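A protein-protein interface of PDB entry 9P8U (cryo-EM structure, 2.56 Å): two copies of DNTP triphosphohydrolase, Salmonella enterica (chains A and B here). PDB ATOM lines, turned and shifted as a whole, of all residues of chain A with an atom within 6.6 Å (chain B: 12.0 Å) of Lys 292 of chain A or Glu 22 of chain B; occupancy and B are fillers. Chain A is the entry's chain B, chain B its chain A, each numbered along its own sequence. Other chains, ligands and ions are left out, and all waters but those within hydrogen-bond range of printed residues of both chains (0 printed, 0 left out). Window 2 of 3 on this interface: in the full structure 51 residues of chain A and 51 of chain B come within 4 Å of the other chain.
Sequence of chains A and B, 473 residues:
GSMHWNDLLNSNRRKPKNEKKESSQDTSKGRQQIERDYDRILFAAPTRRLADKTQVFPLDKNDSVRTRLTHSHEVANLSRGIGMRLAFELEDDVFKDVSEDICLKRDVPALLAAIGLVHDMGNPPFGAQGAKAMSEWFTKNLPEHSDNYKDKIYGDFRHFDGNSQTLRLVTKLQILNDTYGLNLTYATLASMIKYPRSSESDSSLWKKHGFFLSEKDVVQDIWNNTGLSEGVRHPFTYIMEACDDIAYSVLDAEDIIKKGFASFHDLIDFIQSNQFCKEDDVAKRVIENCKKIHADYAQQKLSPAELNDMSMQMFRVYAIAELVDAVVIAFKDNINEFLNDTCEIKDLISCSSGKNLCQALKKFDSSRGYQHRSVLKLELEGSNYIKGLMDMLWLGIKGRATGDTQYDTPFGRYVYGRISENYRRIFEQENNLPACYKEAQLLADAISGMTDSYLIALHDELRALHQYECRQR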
ATOM      1  N   ILE A 287      -6.112 -16.637   5.514  1.00  0.00           N
ATOM      2  CA  ILE A 287      -6.560 -15.597   4.591  1.00  0.00           C
ATOM      3  C   ILE A 287      -5.656 -14.375   4.681  1.00  0.00           C
ATOM      4  O   ILE A 287      -5.290 -13.780   3.659  1.00  0.00           O
ATOM      5  CB  ILE A 287      -8.031 -15.235   4.867  1.00  0.00           C
ATOM      6  CG1 ILE A 287      -8.943 -16.421   4.550  1.00  0.00           C
ATOM      7  CG2 ILE A 287      -8.445 -14.024   4.051  1.00  0.00           C
ATOM      8  CD1 ILE A 287      -8.831 -16.911   3.133  1.00  0.00           C
ATOM      9  N   GLU A 288      -5.291 -13.973   5.901  1.00  0.00           N
ATOM     10  CA  GLU A 288      -4.433 -12.804   6.067  1.00  0.00           C
ATOM     11  C   GLU A 288      -3.075 -13.024   5.418  1.00  0.00           C
ATOM     12  O   GLU A 288      -2.564 -12.148   4.711  1.00  0.00           O
ATOM     13  CB  GLU A 288      -4.271 -12.477   7.551  1.00  0.00           C
ATOM     14  CG  GLU A 288      -5.507 -11.880   8.196  1.00  0.00           C
ATOM     15  CD  GLU A 288      -5.518 -12.060   9.701  1.00  0.00           C
ATOM     16  OE1 GLU A 288      -4.528 -12.592  10.244  1.00  0.00           O
ATOM     17  OE2 GLU A 288      -6.518 -11.670  10.340  1.00  0.00           O
ATOM     18  N   ASN A 289      -2.475 -14.195   5.644  1.00  0.00           N
ATOM     19  CA  ASN A 289      -1.180 -14.484   5.037  1.00  0.00           C
ATOM     20  C   ASN A 289      -1.281 -14.525   3.518  1.00  0.00           C
ATOM     21  O   ASN A 289      -0.402 -14.009   2.814  1.00  0.00           O
ATOM     22  CB  ASN A 289      -0.633 -15.803   5.578  1.00  0.00           C
ATOM     23  CG  ASN A 289      -0.339 -15.745   7.061  1.00  0.00           C
ATOM     24  OD1 ASN A 289      -0.507 -14.705   7.696  1.00  0.00           O
ATOM     25  ND2 ASN A 289       0.100 -16.863   7.622  1.00  0.00           N
ATOM     26  N   CYS A 290      -2.350 -15.130   2.994  1.00  0.00           N
ATOM     27  CA  CYS A 290      -2.520 -15.205   1.549  1.00  0.00           C
ATOM     28  C   CYS A 290      -2.653 -13.819   0.937  1.00  0.00           C
ATOM     29  O   CYS A 290      -2.033 -13.531  -0.089  1.00  0.00           O
ATOM     30  CB  CYS A 290      -3.736 -16.060   1.207  1.00  0.00           C
ATOM     31  SG  CYS A 290      -3.498 -17.815   1.507  1.00  0.00           S
ATOM     32  N   LYS A 291      -3.452 -12.946   1.552  1.00  0.00           N
ATOM     33  CA  LYS A 291      -3.597 -11.591   1.026  1.00  0.00           C
ATOM     34  C   LYS A 291      -2.292 -10.811   1.131  1.00  0.00           C
ATOM     35  O   LYS A 291      -1.924 -10.071   0.207  1.00  0.00           O
ATOM     36  CB  LYS A 291      -4.721 -10.863   1.760  1.00  0.00           C
ATOM     37  CG  LYS A 291      -6.103 -11.411   1.456  1.00  0.00           C
ATOM     38  CD  LYS A 291      -7.187 -10.540   2.061  1.00  0.00           C
ATOM     39  CE  LYS A 291      -8.563 -10.960   1.573  1.00  0.00           C
ATOM     40  NZ  LYS A 291      -9.626 -10.042   2.062  1.00  0.00           N
ATOM     41  N   LYS A 292      -1.578 -10.968   2.248  1.00  0.00           N
ATOM     42  CA  LYS A 292      -0.318 -10.261   2.435  1.00  0.00           C
ATOM     43  C   LYS A 292       0.700 -10.663   1.378  1.00  0.00           C
ATOM     44  O   LYS A 292       1.423  -9.813   0.847  1.00  0.00           O
ATOM     45  CB  LYS A 292       0.226 -10.534   3.836  1.00  0.00           C
ATOM     46  CG  LYS A 292       1.505  -9.795   4.167  1.00  0.00           C
ATOM     47  CD  LYS A 292       1.815  -9.889   5.650  1.00  0.00           C
ATOM     48  CE  LYS A 292       3.081  -9.127   6.001  1.00  0.00           C
ATOM     49  NZ  LYS A 292       3.357  -9.156   7.463  1.00  0.00           N
ATOM     50  N   ILE A 293       0.772 -11.954   1.056  1.00  0.00           N
ATOM     51  CA  ILE A 293       1.723 -12.379   0.036  1.00  0.00           C
ATOM     52  C   ILE A 293       1.199 -12.063  -1.364  1.00  0.00           C
ATOM     53  O   ILE A 293       1.987 -11.823  -2.288  1.00  0.00           O
ATOM     54  CB  ILE A 293       2.053 -13.873   0.206  1.00  0.00           C
ATOM     55  CG1 ILE A 293       3.406 -14.192  -0.421  1.00  0.00           C
ATOM     56  CG2 ILE A 293       0.971 -14.749  -0.402  1.00  0.00           C
ATOM     57  CD1 ILE A 293       4.577 -13.914   0.491  1.00  0.00           C
ATOM     58  N   HIS A 294      -0.125 -12.017  -1.539  1.00  0.00           N
ATOM     59  CA  HIS A 294      -0.701 -11.755  -2.851  1.00  0.00           C
ATOM     60  C   HIS A 294      -0.484 -10.310  -3.268  1.00  0.00           C
ATOM     61  O   HIS A 294      -0.295 -10.027  -4.453  1.00  0.00           O
ATOM     62  CB  HIS A 294      -2.191 -12.093  -2.840  1.00  0.00           C
ATOM     63  CG  HIS A 294      -2.874 -11.866  -4.152  1.00  0.00           C
ATOM     64  ND1 HIS A 294      -2.941 -12.831  -5.133  1.00  0.00           N
ATOM     65  CD2 HIS A 294      -3.528 -10.786  -4.642  1.00  0.00           C
ATOM     66  CE1 HIS A 294      -3.603 -12.355  -6.172  1.00  0.00           C
ATOM     67  NE2 HIS A 294      -3.970 -11.116  -5.900  1.00  0.00           N
ATOM     68  N   ALA A 295      -0.512  -9.380  -2.312  1.00  0.00           N
ATOM     69  CA  ALA A 295      -0.200  -7.992  -2.643  1.00  0.00           C
ATOM     70  C   ALA A 295       1.222  -7.866  -3.185  1.00  0.00           C
ATOM     71  O   ALA A 295       1.452  -7.266  -4.246  1.00  0.00           O
ATOM     72  CB  ALA A 295      -0.391  -7.105  -1.414  1.00  0.00           C
ATOM     73  N   ASP A 296       2.188  -8.458  -2.478  1.00  0.00           N
ATOM     74  CA  ASP A 296       3.577  -8.408  -2.920  1.00  0.00           C
ATOM     75  C   ASP A 296       3.748  -9.084  -4.274  1.00  0.00           C
ATOM     76  O   ASP A 296       4.510  -8.610  -5.123  1.00  0.00           O
ATOM     77  CB  ASP A 296       4.476  -9.066  -1.874  1.00  0.00           C
ATOM     78  CG  ASP A 296       5.943  -9.042  -2.260  1.00  0.00           C
ATOM     79  OD1 ASP A 296       6.335  -8.197  -3.091  1.00  0.00           O
ATOM     80  OD2 ASP A 296       6.707  -9.876  -1.731  1.00  0.00           O
ATOM     81  N   TYR A 297       3.049 -10.197  -4.492  1.00  0.00           N
ATOM     82  CA  TYR A 297       3.158 -10.899  -5.767  1.00  0.00           C
ATOM     83  C   TYR A 297       2.534 -10.088  -6.896  1.00  0.00           C
ATOM     84  O   TYR A 297       3.016 -10.111  -8.034  1.00  0.00           O
ATOM     85  CB  TYR A 297       2.517 -12.277  -5.637  1.00  0.00           C
ATOM     86  CG  TYR A 297       3.370 -13.230  -4.833  1.00  0.00           C
ATOM     87  CD1 TYR A 297       4.607 -12.833  -4.340  1.00  0.00           C
ATOM     88  CD2 TYR A 297       2.919 -14.497  -4.511  1.00  0.00           C
ATOM     89  CE1 TYR A 297       5.389 -13.686  -3.593  1.00  0.00           C
ATOM     90  CE2 TYR A 297       3.693 -15.356  -3.756  1.00  0.00           C
ATOM     91  CZ  TYR A 297       4.927 -14.948  -3.304  1.00  0.00           C
ATOM     92  OH  TYR A 297       5.698 -15.804  -2.552  1.00  0.00           O
ATOM     93  N   LYS B  17      17.081 -13.373   4.256  1.00  0.00           N
ATOM     94  CA  LYS B  17      15.940 -13.606   5.130  1.00  0.00           C
ATOM     95  C   LYS B  17      15.105 -12.340   5.255  1.00  0.00           C
ATOM     96  O   LYS B  17      15.638 -11.248   5.472  1.00  0.00           O
ATOM     97  CB  LYS B  17      16.415 -14.072   6.503  1.00  0.00           C
ATOM     98  CG  LYS B  17      15.339 -14.755   7.328  1.00  0.00           C
ATOM     99  CD  LYS B  17      15.846 -16.061   7.916  1.00  0.00           C
ATOM    100  CE  LYS B  17      17.172 -15.867   8.633  1.00  0.00           C
ATOM    101  NZ  LYS B  17      17.065 -14.881   9.745  1.00  0.00           N
ATOM    102  N   ASN B  18      13.791 -12.489   5.113  1.00  0.00           N
ATOM    103  CA  ASN B  18      12.889 -11.349   5.207  1.00  0.00           C
ATOM    104  C   ASN B  18      12.704 -10.964   6.669  1.00  0.00           C
ATOM    105  O   ASN B  18      12.183 -11.751   7.466  1.00  0.00           O
ATOM    106  CB  ASN B  18      11.547 -11.686   4.563  1.00  0.00           C
ATOM    107  CG  ASN B  18      10.650 -10.474   4.417  1.00  0.00           C
ATOM    108  OD1 ASN B  18      11.057  -9.346   4.701  1.00  0.00           O
ATOM    109  ND2 ASN B  18       9.419 -10.699   3.973  1.00  0.00           N
ATOM    110  N   GLU B  19      13.129  -9.753   7.019  1.00  0.00           N
ATOM    111  CA  GLU B  19      13.042  -9.272   8.391  1.00  0.00           C
ATOM    112  C   GLU B  19      11.642  -8.805   8.767  1.00  0.00           C
ATOM    113  O   GLU B  19      11.402  -8.508   9.942  1.00  0.00           O
ATOM    114  CB  GLU B  19      14.042  -8.135   8.616  1.00  0.00           C
ATOM    115  CG  GLU B  19      15.486  -8.502   8.304  1.00  0.00           C
ATOM    116  CD  GLU B  19      15.833  -8.327   6.837  1.00  0.00           C
ATOM    117  OE1 GLU B  19      14.951  -7.895   6.064  1.00  0.00           O
ATOM    118  OE2 GLU B  19      16.984  -8.624   6.456  1.00  0.00           O
ATOM    119  N   LYS B  20      10.722  -8.735   7.808  1.00  0.00           N
ATOM    120  CA  LYS B  20       9.353  -8.308   8.062  1.00  0.00           C
ATOM    121  C   LYS B  20       8.429  -9.476   8.378  1.00  0.00           C
ATOM    122  O   LYS B  20       7.239  -9.263   8.627  1.00  0.00           O
ATOM    123  CB  LYS B  20       8.807  -7.521   6.866  1.00  0.00           C
ATOM    124  CG  LYS B  20       9.141  -6.025   6.848  1.00  0.00           C
ATOM    125  CD  LYS B  20      10.629  -5.735   7.004  1.00  0.00           C
ATOM    126  CE  LYS B  20      11.424  -6.253   5.814  1.00  0.00           C
ATOM    127  NZ  LYS B  20      12.875  -5.936   5.932  1.00  0.00           N
ATOM    128  N   LYS B  21       8.946 -10.702   8.369  1.00  0.00           N
ATOM    129  CA  LYS B  21       8.123 -11.865   8.666  1.00  0.00           C
ATOM    130  C   LYS B  21       7.705 -11.866  10.130  1.00  0.00           C
ATOM    131  O   LYS B  21       8.497 -11.546  11.020  1.00  0.00           O
ATOM    132  CB  LYS B  21       8.878 -13.152   8.337  1.00  0.00           C
ATOM    133  CG  LYS B  21       9.007 -13.437   6.852  1.00  0.00           C
ATOM    134  CD  LYS B  21       7.660 -13.363   6.154  1.00  0.00           C
ATOM    135  CE  LYS B  21       7.794 -13.654   4.670  1.00  0.00           C
ATOM    136  NZ  LYS B  21       6.502 -13.481   3.950  1.00  0.00           N
ATOM    137  N   GLU B  22       6.453 -12.229  10.374  1.00  0.00           N
ATOM    138  CA  GLU B  22       5.904 -12.332  11.716  1.00  0.00           C
ATOM    139  C   GLU B  22       5.783 -13.797  12.115  1.00  0.00           C
ATOM    140  O   GLU B  22       5.935 -14.707  11.295  1.00  0.00           O
ATOM    141  CB  GLU B  22       4.541 -11.639  11.800  1.00  0.00           C
ATOM    142  CG  GLU B  22       4.519 -10.251  11.186  1.00  0.00           C
ATOM    143  CD  GLU B  22       3.127  -9.824  10.767  1.00  0.00           C
ATOM    144  OE1 GLU B  22       2.530 -10.502   9.905  1.00  0.00           O
ATOM    145  OE2 GLU B  22       2.630  -8.809  11.298  1.00  0.00           O
ATOM    146  N   SER B  23       5.506 -14.018  13.401  1.00  0.00           N
ATOM    147  CA  SER B  23       5.358 -15.379  13.902  1.00  0.00           C
ATOM    148  C   SER B  23       4.155 -16.088  13.294  1.00  0.00           C
ATOM    149  O   SER B  23       4.126 -17.323  13.272  1.00  0.00           O
ATOM    150  CB  SER B  23       5.239 -15.367  15.425  1.00  0.00           C
ATOM    151  OG  SER B  23       3.990 -14.840  15.835  1.00  0.00           O
ATOM    152  N   SER B  24       3.168 -15.341  12.802  1.00  0.00           N
ATOM    153  CA  SER B  24       2.003 -15.945  12.171  1.00  0.00           C
ATOM    154  C   SER B  24       2.287 -16.451  10.764  1.00  0.00           C
ATOM    155  O   SER B  24       1.519 -17.273  10.255  1.00  0.00           O
ATOM    156  CB  SER B  24       0.849 -14.942  12.129  1.00  0.00           C
ATOM    157  OG  SER B  24       1.165 -13.839  11.300  1.00  0.00           O
ATOM    158  N   GLN B  25       3.359 -15.984  10.128  1.00  0.00           N
ATOM    159  CA  GLN B  25       3.728 -16.426   8.790  1.00  0.00           C
ATOM    160  C   GLN B  25       4.767 -17.537   8.809  1.00  0.00           C
ATOM    161  O   GLN B  25       5.213 -17.972   7.743  1.00  0.00           O
ATOM    162  CB  GLN B  25       4.243 -15.247   7.963  1.00  0.00           C
ATOM    163  CG  GLN B  25       3.464 -13.963   8.157  1.00  0.00           C
ATOM    164  CD  GLN B  25       3.995 -12.832   7.303  1.00  0.00           C
ATOM    165  OE1 GLN B  25       4.442 -11.808   7.819  1.00  0.00           O
ATOM    166  NE2 GLN B  25       3.952 -13.013   5.989  1.00  0.00           N
ATOM    167  N   ASP B  26       5.171 -18.000   9.989  1.00  0.00           N
ATOM    168  CA  ASP B  26       6.136 -19.086  10.066  1.00  0.00           C
ATOM    169  C   ASP B  26       5.530 -20.367   9.508  1.00  0.00           C
ATOM    170  O   ASP B  26       4.390 -20.722   9.818  1.00  0.00           O
ATOM    171  CB  ASP B  26       6.588 -19.298  11.510  1.00  0.00           C
ATOM    172  CG  ASP B  26       7.342 -20.597  11.698  1.00  0.00           C
ATOM    173  OD1 ASP B  26       8.391 -20.774  11.044  1.00  0.00           O
ATOM    174  OD2 ASP B  26       6.887 -21.441  12.496  1.00  0.00           O
ATOM    175  N   THR B  27       6.306 -21.063   8.681  1.00  0.00           N
ATOM    176  CA  THR B  27       5.836 -22.252   7.991  1.00  0.00           C
ATOM    177  C   THR B  27       6.621 -23.502   8.375  1.00  0.00           C
ATOM    178  O   THR B  27       6.162 -24.613   8.088  1.00  0.00           O
ATOM    179  CB  THR B  27       5.902 -22.025   6.469  1.00  0.00           C
ATOM    180  OG1 THR B  27       5.136 -20.861   6.138  1.00  0.00           O
ATOM    181  CG2 THR B  27       5.311 -23.192   5.694  1.00  0.00           C
ATOM    182  N   SER B  28       7.759 -23.353   9.057  1.00  0.00           N
ATOM    183  CA  SER B  28       8.579 -24.508   9.411  1.00  0.00           C
ATOM    184  C   SER B  28       7.784 -25.524  10.222  1.00  0.00           C
ATOM    185  O   SER B  28       7.793 -26.721   9.915  1.00  0.00           O
ATOM    186  CB  SER B  28       9.814 -24.052  10.187  1.00  0.00           C
ATOM    187  OG  SER B  28      10.634 -23.216   9.392  1.00  0.00           O
ATOM    188  N   LYS B  29       7.076 -25.059  11.251  1.00  0.00           N
ATOM    189  CA  LYS B  29       6.245 -25.916  12.095  1.00  0.00           C
ATOM    190  C   LYS B  29       7.057 -27.074  12.670  1.00  0.00           C
ATOM    191  O   LYS B  29       6.668 -28.241  12.596  1.00  0.00           O
ATOM    192  CB  LYS B  29       5.027 -26.428  11.323  1.00  0.00           C
ATOM    193  CG  LYS B  29       3.927 -25.395  11.125  1.00  0.00           C
ATOM    194  CD  LYS B  29       3.890 -24.389  12.262  1.00  0.00           C
ATOM    195  CE  LYS B  29       2.942 -23.244  11.955  1.00  0.00           C
ATOM    196  NZ  LYS B  29       1.568 -23.729  11.662  1.00  0.00           N
ATOM    197  N   ARG B  36      12.481 -29.245   4.903  1.00  0.00           N
ATOM    198  CA  ARG B  36      11.714 -28.289   4.114  1.00  0.00           C
ATOM    199  C   ARG B  36      12.161 -28.284   2.661  1.00  0.00           C
ATOM    200  O   ARG B  36      11.336 -28.104   1.764  1.00  0.00           O
ATOM    201  CB  ARG B  36      11.835 -26.890   4.715  1.00  0.00           C
ATOM    202  CG  ARG B  36      11.441 -26.809   6.176  1.00  0.00           C
ATOM    203  CD  ARG B  36      11.412 -25.374   6.656  1.00  0.00           C
ATOM    204  NE  ARG B  36      10.635 -24.522   5.766  1.00  0.00           N
ATOM    205  CZ  ARG B  36      10.625 -23.198   5.819  1.00  0.00           C
ATOM    206  NH1 ARG B  36      11.355 -22.538   6.701  1.00  0.00           N
ATOM    207  NH2 ARG B  36       9.863 -22.520   4.967  1.00  0.00           N
ATOM    208  N   LEU B 176       8.400 -17.074 -10.063  1.00  0.00           N
ATOM    209  CA  LEU B 176       8.963 -15.810  -9.612  1.00  0.00           C
ATOM    210  C   LEU B 176      10.383 -15.660 -10.138  1.00  0.00           C
ATOM    211  O   LEU B 176      11.201 -16.577 -10.016  1.00  0.00           O
ATOM    212  CB  LEU B 176       8.952 -15.729  -8.087  1.00  0.00           C
ATOM    213  CG  LEU B 176       7.613 -15.429  -7.413  1.00  0.00           C
ATOM    214  CD1 LEU B 176       7.839 -14.727  -6.088  1.00  0.00           C
ATOM    215  CD2 LEU B 176       6.723 -14.593  -8.318  1.00  0.00           C
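The side-chain amino group (NZ) of Lys 292 of chain A is in salt-bridge range of the side-chain carboxylate (OE1) of Glu 22 of chain B, at 2.9 Å. O of Ser 24 of chain B sits at hydrogen-bond distance from ND2 of Asn 289 of chain A, 3.0 Å away. The side-chain amino group (NZ) of Lys 292 of chain A is in hydrogen-bond range of the side-chain amide oxygen (OE1) of Gln 25 of chain B, at 2.9 Å.
No position is printed for both chains. Of the 6 pairs that touch across the chains among the printed residues, none has its exchanged pair printed and touching as well.
Asn 289 of chain A touches just these residues of chain B: Ser 24 (3.0 Å) and Gln 25 (3.8 Å). Lys 292 of chain A touches just these residues of chain B: Glu 22 and Gln 25. Of the printed residues of chain B, Ile 293 of chain A touches Lys 21 (3.98 Å). His 294 of chain A touches none of the printed residues of chain B. No residue of chain B comes within 4 Å of Ala 295 of chain A. No residue of chain B comes within 4 Å of Asp 296 of chain A. Of chain A, only Lys 292 (2.9 Å) comes within 4 Å of Glu 22 of chain B. Lys 29 of chain B touches none of the printed residues of chain A. Of the printed residues of chain A, Leu 176 of chain B touches Tyr 297 (3.6 Å). The nearest residue of chain A that does not touch Glu 22 of chain B is Asn 289 of chain A (5.6 Å). The nearest printed residue of chain A that does not touch Leu 176 of chain B is Asp 296 of chain A (6.6 Å).
The side-chain amino group (NZ) of Lys 21 of chain B sits close to the side-chain amide nitrogen (NE2) of Gln 25 of chain B (3.3 Å). The side-chain amide oxygen (OE1) of Gln 25 of chain B lies close to the side-chain carboxylate (OE1) of Glu 22 of chain B, 3.1 Å away. The backbone carbonyl oxygen (O) of Gln 25 of chain B sits at hydrogen-bond distance from the side-chain hydroxyl (OG1) of Thr 27 of chain B (3.3 Å).
Among the printed residues, pairs that only touch across the chains: Asn 289 of chain A with Gln 25 of chain B, Ile 293 of chain A with Lys 21 of chain B and Tyr 297 of chain A with Leu 176 of chain B.
Hydrophobic or aromatic side chains of chain B within 4 Å of the printed part of chain A: Leu 176. Along chain B the printed residues that touch a printed residue of chain A span positions 21 to 176. Hydrophobic or aromatic side chains of chain A that line the printed part of chain B: Ile 293 and Tyr 297. Among the printed residues, 6 pairs touch across the chains. Among the printed residues, Asp or Glu carboxylates within 4 Å of a Lys or Arg side-chain nitrogen of the other chain: Lys 292 of chain A with Glu 22 of chain B.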
